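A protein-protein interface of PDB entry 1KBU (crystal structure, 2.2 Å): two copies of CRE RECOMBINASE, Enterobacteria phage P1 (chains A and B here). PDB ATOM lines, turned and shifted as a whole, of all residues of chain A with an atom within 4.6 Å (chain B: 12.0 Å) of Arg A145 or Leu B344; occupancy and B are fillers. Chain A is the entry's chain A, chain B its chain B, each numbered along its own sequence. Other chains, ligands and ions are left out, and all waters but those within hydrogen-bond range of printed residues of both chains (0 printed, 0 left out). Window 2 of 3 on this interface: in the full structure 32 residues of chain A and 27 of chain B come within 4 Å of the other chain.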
ATOM      1  N   PHE A 143       8.942  -8.781 -28.151  1.00  0.00           N
ATOM      2  CA  PHE A 143       9.960  -7.901 -28.699  1.00  0.00           C
ATOM      3  C   PHE A 143      11.145  -8.843 -28.709  1.00  0.00           C
ATOM      4  O   PHE A 143      11.883  -8.957 -27.731  1.00  0.00           O
ATOM      5  CB  PHE A 143      10.236  -6.694 -27.814  1.00  0.00           C
ATOM      6  CG  PHE A 143      11.336  -5.823 -28.332  1.00  0.00           C
ATOM      7  CD1 PHE A 143      11.108  -4.973 -29.404  1.00  0.00           C
ATOM      8  CD2 PHE A 143      12.600  -5.873 -27.768  1.00  0.00           C
ATOM      9  CE1 PHE A 143      12.121  -4.177 -29.905  1.00  0.00           C
ATOM     10  CE2 PHE A 143      13.618  -5.086 -28.263  1.00  0.00           C
ATOM     11  CZ  PHE A 143      13.377  -4.232 -29.329  1.00  0.00           C
ATOM     12  N   GLU A 144      11.244  -9.591 -29.801  1.00  0.00           N
ATOM     13  CA  GLU A 144      12.268 -10.605 -29.963  1.00  0.00           C
ATOM     14  C   GLU A 144      13.486 -10.069 -30.718  1.00  0.00           C
ATOM     15  O   GLU A 144      13.463  -8.948 -31.232  1.00  0.00           O
ATOM     16  CB  GLU A 144      11.662 -11.830 -30.656  1.00  0.00           C
ATOM     17  CG  GLU A 144      10.147 -11.971 -30.505  1.00  0.00           C
ATOM     18  CD  GLU A 144       9.709 -13.424 -30.456  1.00  0.00           C
ATOM     19  OE1 GLU A 144       9.859 -14.041 -29.387  1.00  0.00           O
ATOM     20  OE2 GLU A 144       9.231 -13.957 -31.483  1.00  0.00           O
ATOM     21  N   ARG A 145      14.550 -10.870 -30.754  1.00  0.00           N
ATOM     22  CA  ARG A 145      15.791 -10.505 -31.431  1.00  0.00           C
ATOM     23  C   ARG A 145      15.558  -9.971 -32.839  1.00  0.00           C
ATOM     24  O   ARG A 145      16.204  -9.010 -33.263  1.00  0.00           O
ATOM     25  CB  ARG A 145      16.742 -11.693 -31.511  1.00  0.00           C
ATOM     26  CG  ARG A 145      17.734 -11.546 -32.642  1.00  0.00           C
ATOM     27  CD  ARG A 145      19.150 -11.647 -32.135  1.00  0.00           C
ATOM     28  NE  ARG A 145      19.613 -10.412 -31.515  1.00  0.00           N
ATOM     29  CZ  ARG A 145      20.734 -10.310 -30.811  1.00  0.00           C
ATOM     30  NH1 ARG A 145      21.513 -11.375 -30.649  1.00  0.00           N
ATOM     31  NH2 ARG A 145      21.093  -9.143 -30.291  1.00  0.00           N
ATOM     32  N   THR A 146      14.656 -10.607 -33.577  1.00  0.00           N
ATOM     33  CA  THR A 146      14.384 -10.149 -34.930  1.00  0.00           C
ATOM     34  C   THR A 146      13.972  -8.693 -34.805  1.00  0.00           C
ATOM     35  O   THR A 146      14.238  -7.874 -35.683  1.00  0.00           O
ATOM     36  CB  THR A 146      13.224 -10.922 -35.569  1.00  0.00           C
ATOM     37  OG1 THR A 146      11.984 -10.341 -35.147  1.00  0.00           O
ATOM     38  CG2 THR A 146      13.265 -12.381 -35.151  1.00  0.00           C
ATOM     39  N   ASP A 147      13.324  -8.377 -33.690  1.00  0.00           N
ATOM     40  CA  ASP A 147      12.858  -7.020 -33.436  1.00  0.00           C
ATOM     41  C   ASP A 147      13.972  -6.052 -33.029  1.00  0.00           C
ATOM     42  O   ASP A 147      14.041  -4.918 -33.504  1.00  0.00           O
ATOM     43  CB  ASP A 147      11.701  -7.039 -32.433  1.00  0.00           C
ATOM     44  CG  ASP A 147      10.437  -7.662 -33.013  1.00  0.00           C
ATOM     45  OD1 ASP A 147       9.838  -7.053 -33.925  1.00  0.00           O
ATOM     46  OD2 ASP A 147      10.033  -8.751 -32.552  1.00  0.00           O
ATOM     47  N   PHE A 148      14.861  -6.530 -32.167  1.00  0.00           N
ATOM     48  CA  PHE A 148      15.994  -5.753 -31.674  1.00  0.00           C
ATOM     49  C   PHE A 148      16.977  -5.424 -32.800  1.00  0.00           C
ATOM     50  O   PHE A 148      17.416  -4.281 -32.935  1.00  0.00           O
ATOM     51  CB  PHE A 148      16.681  -6.540 -30.555  1.00  0.00           C
ATOM     52  CG  PHE A 148      17.722  -5.762 -29.797  1.00  0.00           C
ATOM     53  CD1 PHE A 148      17.511  -4.445 -29.407  1.00  0.00           C
ATOM     54  CD2 PHE A 148      18.924  -6.367 -29.456  1.00  0.00           C
ATOM     55  CE1 PHE A 148      18.488  -3.747 -28.700  1.00  0.00           C
ATOM     56  CE2 PHE A 148      19.899  -5.681 -28.748  1.00  0.00           C
ATOM     57  CZ  PHE A 148      19.684  -4.367 -28.374  1.00  0.00           C
ATOM     58  N   ASP A 149      17.298  -6.420 -33.623  1.00  0.00           N
ATOM     59  CA  ASP A 149      18.212  -6.238 -34.748  1.00  0.00           C
ATOM     60  C   ASP A 149      17.691  -5.189 -35.710  1.00  0.00           C
ATOM     61  O   ASP A 149      18.404  -4.264 -36.097  1.00  0.00           O
ATOM     62  CB  ASP A 149      18.369  -7.555 -35.500  1.00  0.00           C
ATOM     63  CG  ASP A 149      19.393  -8.461 -34.862  1.00  0.00           C
ATOM     64  OD1 ASP A 149      20.145  -7.994 -33.980  1.00  0.00           O
ATOM     65  OD2 ASP A 149      19.447  -9.647 -35.243  1.00  0.00           O
ATOM     66  N   ARG A 152      17.728  -2.017 -34.041  1.00  0.00           N
ATOM     67  CA  ARG A 152      19.152  -1.732 -33.974  1.00  0.00           C
ATOM     68  C   ARG A 152      19.602  -1.253 -35.356  1.00  0.00           C
ATOM     69  O   ARG A 152      20.439  -0.362 -35.473  1.00  0.00           O
ATOM     70  CB  ARG A 152      19.885  -3.028 -33.635  1.00  0.00           C
ATOM     71  CG  ARG A 152      20.901  -2.921 -32.523  1.00  0.00           C
ATOM     72  CD  ARG A 152      22.092  -3.814 -32.828  1.00  0.00           C
ATOM     73  NE  ARG A 152      21.928  -5.150 -32.269  1.00  0.00           N
ATOM     74  CZ  ARG A 152      22.311  -5.483 -31.042  1.00  0.00           C
ATOM     75  NH1 ARG A 152      22.868  -4.568 -30.257  1.00  0.00           N
ATOM     76  NH2 ARG A 152      22.123  -6.716 -30.590  1.00  0.00           N
ATOM     77  N   TYR A 174      15.869  -6.311 -23.214  1.00  0.00           N
ATOM     78  CA  TYR A 174      15.907  -7.600 -23.902  1.00  0.00           C
ATOM     79  C   TYR A 174      17.049  -8.487 -23.405  1.00  0.00           C
ATOM     80  O   TYR A 174      16.828  -9.608 -22.941  1.00  0.00           O
ATOM     81  CB  TYR A 174      15.990  -7.420 -25.415  1.00  0.00           C
ATOM     82  CG  TYR A 174      16.089  -8.732 -26.161  1.00  0.00           C
ATOM     83  CD1 TYR A 174      14.948  -9.382 -26.618  1.00  0.00           C
ATOM     84  CD2 TYR A 174      17.322  -9.330 -26.390  1.00  0.00           C
ATOM     85  CE1 TYR A 174      15.031 -10.582 -27.307  1.00  0.00           C
ATOM     86  CE2 TYR A 174      17.417 -10.534 -27.081  1.00  0.00           C
ATOM     87  CZ  TYR A 174      16.263 -11.153 -27.537  1.00  0.00           C
ATOM     88  OH  TYR A 174      16.326 -12.347 -28.226  1.00  0.00           O
ATOM     89  N   ALA A 301      12.486 -12.269 -25.134  1.00  0.00           N
ATOM     90  CA  ALA A 301      13.736 -12.846 -24.645  1.00  0.00           C
ATOM     91  C   ALA A 301      13.510 -14.328 -24.387  1.00  0.00           C
ATOM     92  O   ALA A 301      14.313 -15.176 -24.786  1.00  0.00           O
ATOM     93  CB  ALA A 301      14.157 -12.148 -23.357  1.00  0.00           C
ATOM     94  N   ASP A 304      12.819 -16.528 -27.550  1.00  0.00           N
ATOM     95  CA  ASP A 304      14.067 -16.687 -28.266  1.00  0.00           C
ATOM     96  C   ASP A 304      14.875 -17.738 -27.537  1.00  0.00           C
ATOM     97  O   ASP A 304      15.422 -18.646 -28.155  1.00  0.00           O
ATOM     98  CB  ASP A 304      14.793 -15.355 -28.351  1.00  0.00           C
ATOM     99  CG  ASP A 304      13.933 -14.299 -28.984  1.00  0.00           C
ATOM    100  OD1 ASP A 304      12.951 -14.672 -29.665  1.00  0.00           O
ATOM    101  OD2 ASP A 304      14.230 -13.101 -28.789  1.00  0.00           O
ATOM    102  N   MET A 305      14.897 -17.614 -26.212  1.00  0.00           N
ATOM    103  CA  MET A 305      15.586 -18.545 -25.318  1.00  0.00           C
ATOM    104  C   MET A 305      14.950 -19.938 -25.340  1.00  0.00           C
ATOM    105  O   MET A 305      15.623 -20.942 -25.076  1.00  0.00           O
ATOM    106  CB  MET A 305      15.684 -17.986 -23.888  1.00  0.00           C
ATOM    107  CG  MET A 305      17.163 -17.864 -23.385  1.00  0.00           C
ATOM    108  SD  MET A 305      17.246 -17.073 -21.789  1.00  0.00           S
ATOM    109  CE  MET A 305      15.473 -16.907 -21.885  1.00  0.00           C
ATOM    110  N   GLY B 339      25.399 -14.432 -18.949  1.00  0.00           N
ATOM    111  CA  GLY B 339      24.799 -15.748 -18.739  1.00  0.00           C
ATOM    112  C   GLY B 339      24.215 -16.365 -20.002  1.00  0.00           C
ATOM    113  O   GLY B 339      24.801 -16.306 -21.084  1.00  0.00           O
ATOM    114  N   ALA B 340      23.048 -16.968 -19.823  1.00  0.00           N
ATOM    115  CA  ALA B 340      22.346 -17.614 -20.912  1.00  0.00           C
ATOM    116  C   ALA B 340      21.973 -16.600 -21.982  1.00  0.00           C
ATOM    117  O   ALA B 340      22.056 -16.909 -23.172  1.00  0.00           O
ATOM    118  CB  ALA B 340      21.095 -18.304 -20.392  1.00  0.00           C
ATOM    119  N   MET B 341      21.527 -15.413 -21.569  1.00  0.00           N
ATOM    120  CA  MET B 341      21.086 -14.385 -22.515  1.00  0.00           C
ATOM    121  C   MET B 341      22.236 -13.742 -23.263  1.00  0.00           C
ATOM    122  O   MET B 341      22.065 -13.112 -24.304  1.00  0.00           O
ATOM    123  CB  MET B 341      20.183 -13.336 -21.855  1.00  0.00           C
ATOM    124  CG  MET B 341      18.716 -13.748 -21.730  1.00  0.00           C
ATOM    125  SD  MET B 341      17.785 -13.923 -23.270  1.00  0.00           S
ATOM    126  CE  MET B 341      18.882 -13.124 -24.457  1.00  0.00           C
ATOM    127  N   VAL B 342      23.426 -13.992 -22.741  1.00  0.00           N
ATOM    128  CA  VAL B 342      24.646 -13.485 -23.335  1.00  0.00           C
ATOM    129  C   VAL B 342      25.330 -14.426 -24.338  1.00  0.00           C
ATOM    130  O   VAL B 342      26.541 -14.350 -24.527  1.00  0.00           O
ATOM    131  CB  VAL B 342      25.630 -13.062 -22.239  1.00  0.00           C
ATOM    132  CG1 VAL B 342      26.539 -11.945 -22.740  1.00  0.00           C
ATOM    133  CG2 VAL B 342      24.868 -12.613 -21.003  1.00  0.00           C
ATOM    134  N   ARG B 343      24.571 -15.302 -24.985  1.00  0.00           N
ATOM    135  CA  ARG B 343      25.126 -16.223 -25.974  1.00  0.00           C
ATOM    136  C   ARG B 343      24.160 -16.156 -27.139  1.00  0.00           C
ATOM    137  O   ARG B 343      24.554 -16.223 -28.304  1.00  0.00           O
ATOM    138  CB  ARG B 343      25.183 -17.639 -25.408  1.00  0.00           C
ATOM    139  CG  ARG B 343      26.252 -17.817 -24.344  1.00  0.00           C
ATOM    140  CD  ARG B 343      25.715 -18.540 -23.117  1.00  0.00           C
ATOM    141  NE  ARG B 343      24.668 -19.507 -23.451  1.00  0.00           N
ATOM    142  CZ  ARG B 343      24.310 -20.529 -22.684  1.00  0.00           C
ATOM    143  NH1 ARG B 343      24.889 -20.715 -21.502  1.00  0.00           N
ATOM    144  NH2 ARG B 343      23.349 -21.354 -23.077  1.00  0.00           N
ATOM    145  N   LEU B 344      22.883 -16.009 -26.801  1.00  0.00           N
ATOM    146  CA  LEU B 344      21.867 -15.839 -27.818  1.00  0.00           C
ATOM    147  C   LEU B 344      22.433 -14.554 -28.389  1.00  0.00           C
ATOM    148  O   LEU B 344      22.953 -14.526 -29.506  1.00  0.00           O
ATOM    149  CB  LEU B 344      20.504 -15.562 -27.182  1.00  0.00           C
ATOM    150  CG  LEU B 344      19.586 -16.780 -27.190  1.00  0.00           C
ATOM    151  CD1 LEU B 344      18.415 -16.580 -26.249  1.00  0.00           C
ATOM    152  CD2 LEU B 344      19.105 -17.079 -28.602  1.00  0.00           C
ATOM    153  N   LEU B 345      22.409 -13.504 -27.579  1.00  0.00           N
ATOM    154  CA  LEU B 345      22.966 -12.255 -28.054  1.00  0.00           C
ATOM    155  C   LEU B 345      24.379 -12.406 -28.607  1.00  0.00           C
ATOM    156  O   LEU B 345      24.605 -12.148 -29.785  1.00  0.00           O
ATOM    157  CB  LEU B 345      22.811 -11.118 -27.044  1.00  0.00           C
ATOM    158  CG  LEU B 345      21.357 -10.800 -26.664  1.00  0.00           C
ATOM    159  CD1 LEU B 345      21.260 -10.281 -25.239  1.00  0.00           C
ATOM    160  CD2 LEU B 345      20.640  -9.859 -27.627  1.00  0.00           C
ATOM    161  N   GLU B 346      25.315 -12.850 -27.773  1.00  0.00           N
ATOM    162  CA  GLU B 346      26.704 -13.035 -28.187  1.00  0.00           C
ATOM    163  C   GLU B 346      26.850 -13.858 -29.469  1.00  0.00           C
ATOM    164  O   GLU B 346      27.688 -13.539 -30.314  1.00  0.00           O
ATOM    165  CB  GLU B 346      27.541 -13.610 -27.038  1.00  0.00           C
ATOM    166  CG  GLU B 346      28.071 -12.575 -26.051  1.00  0.00           C
ATOM    167  CD  GLU B 346      29.122 -11.683 -26.646  1.00  0.00           C
ATOM    168  OE1 GLU B 346      29.309 -11.653 -27.880  1.00  0.00           O
ATOM    169  OE2 GLU B 346      29.671 -10.941 -25.854  1.00  0.00           O
ATOM    170  N   ASP B 347      26.030 -14.898 -29.602  1.00  0.00           N
ATOM    171  CA  ASP B 347      26.041 -15.764 -30.777  1.00  0.00           C
ATOM    172  C   ASP B 347      27.138 -16.824 -30.797  1.00  0.00           C
ATOM    173  O   ASP B 347      27.004 -17.859 -31.452  1.00  0.00           O
ATOM    174  CB  ASP B 347      26.026 -14.947 -32.063  1.00  0.00           C
ATOM    175  CG  ASP B 347      24.635 -14.711 -32.549  1.00  0.00           C
ATOM    176  OD1 ASP B 347      23.744 -14.557 -31.692  1.00  0.00           O
ATOM    177  OD2 ASP B 347      24.417 -14.703 -33.775  1.00  0.00           O
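Of chain B, only Leu B344 and Leu B345 come within 4 Å of Arg A145. Of chain A, only Arg A145 (3.6 Å), Asp A304 (3.9 Å) and Met A305 (3.4 Å) come within 4 Å of Leu B344. Glu A144 touches none of the printed residues of chain B. Thr A146 touches none of the printed residues of chain B. Asp A147 touches none of the printed residues of chain B. No residue of chain B comes within 4 Å of Phe A148. Asp A149 touches none of the printed residues of chain B. Of chain B, only Met B341 and Leu B344 come within 4 Å of Met A305. Of the printed residues of chain B, Ala A301 touches Met B341 (3.99 Å). Of the printed residues of chain B, Tyr A174 touches Met B341 and Leu B345. Printed residues of chain A within 4 Å of Leu B345: Arg A145 and Tyr A174. Ala B340 touches none of the printed residues of chain A. The nearest printed residue of chain A that does not touch Met B341 is Asp A304 (6.1 Å).
No position is printed for both chains.
The backbone NH (N) of Arg A145 sits at hydrogen-bond distance from the side-chain carboxylate (OD2) of Asp A304, 3.0 Å away. The backbone NH (N) of Arg A145 sits close to the side-chain hydroxyl (OH) of Tyr A174, at 3.4 Å. The guanidinium group (NH2) of Arg A145 lies close to the guanidinium group (NH2) of Arg A152 (2.7 Å). The guanidinium group (NE) of Arg A145 lies within salt-bridge range of the side-chain carboxylate (OD1) of Asp A149 (3.5 Å).
Hydrophobic or aromatic side chains of chain A within 4 Å of the printed part of chain B: Tyr A174 and Met A305. Hydrophobic or aromatic side chains of chain B within 4 Å of the printed part of chain A: Met B341, Leu B344 and Leu B345. Among the printed residues, 8 pairs touch across the chains.
O of Leu B345 lies close to NH1 of Arg A145, at 3.3 Å. The side-chain sulfur of Met A305 lies close to the side-chain sulfur of Met B341, at 3.5 Å.
Among the printed residues, pairs that only touch across the chains: Tyr A174 with Leu B345, Met A305 with Leu B344, Arg A145 with Leu B344, Asp A304 with Leu B344, Tyr A174 with Met B341 and Ala A301 with Met B341.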
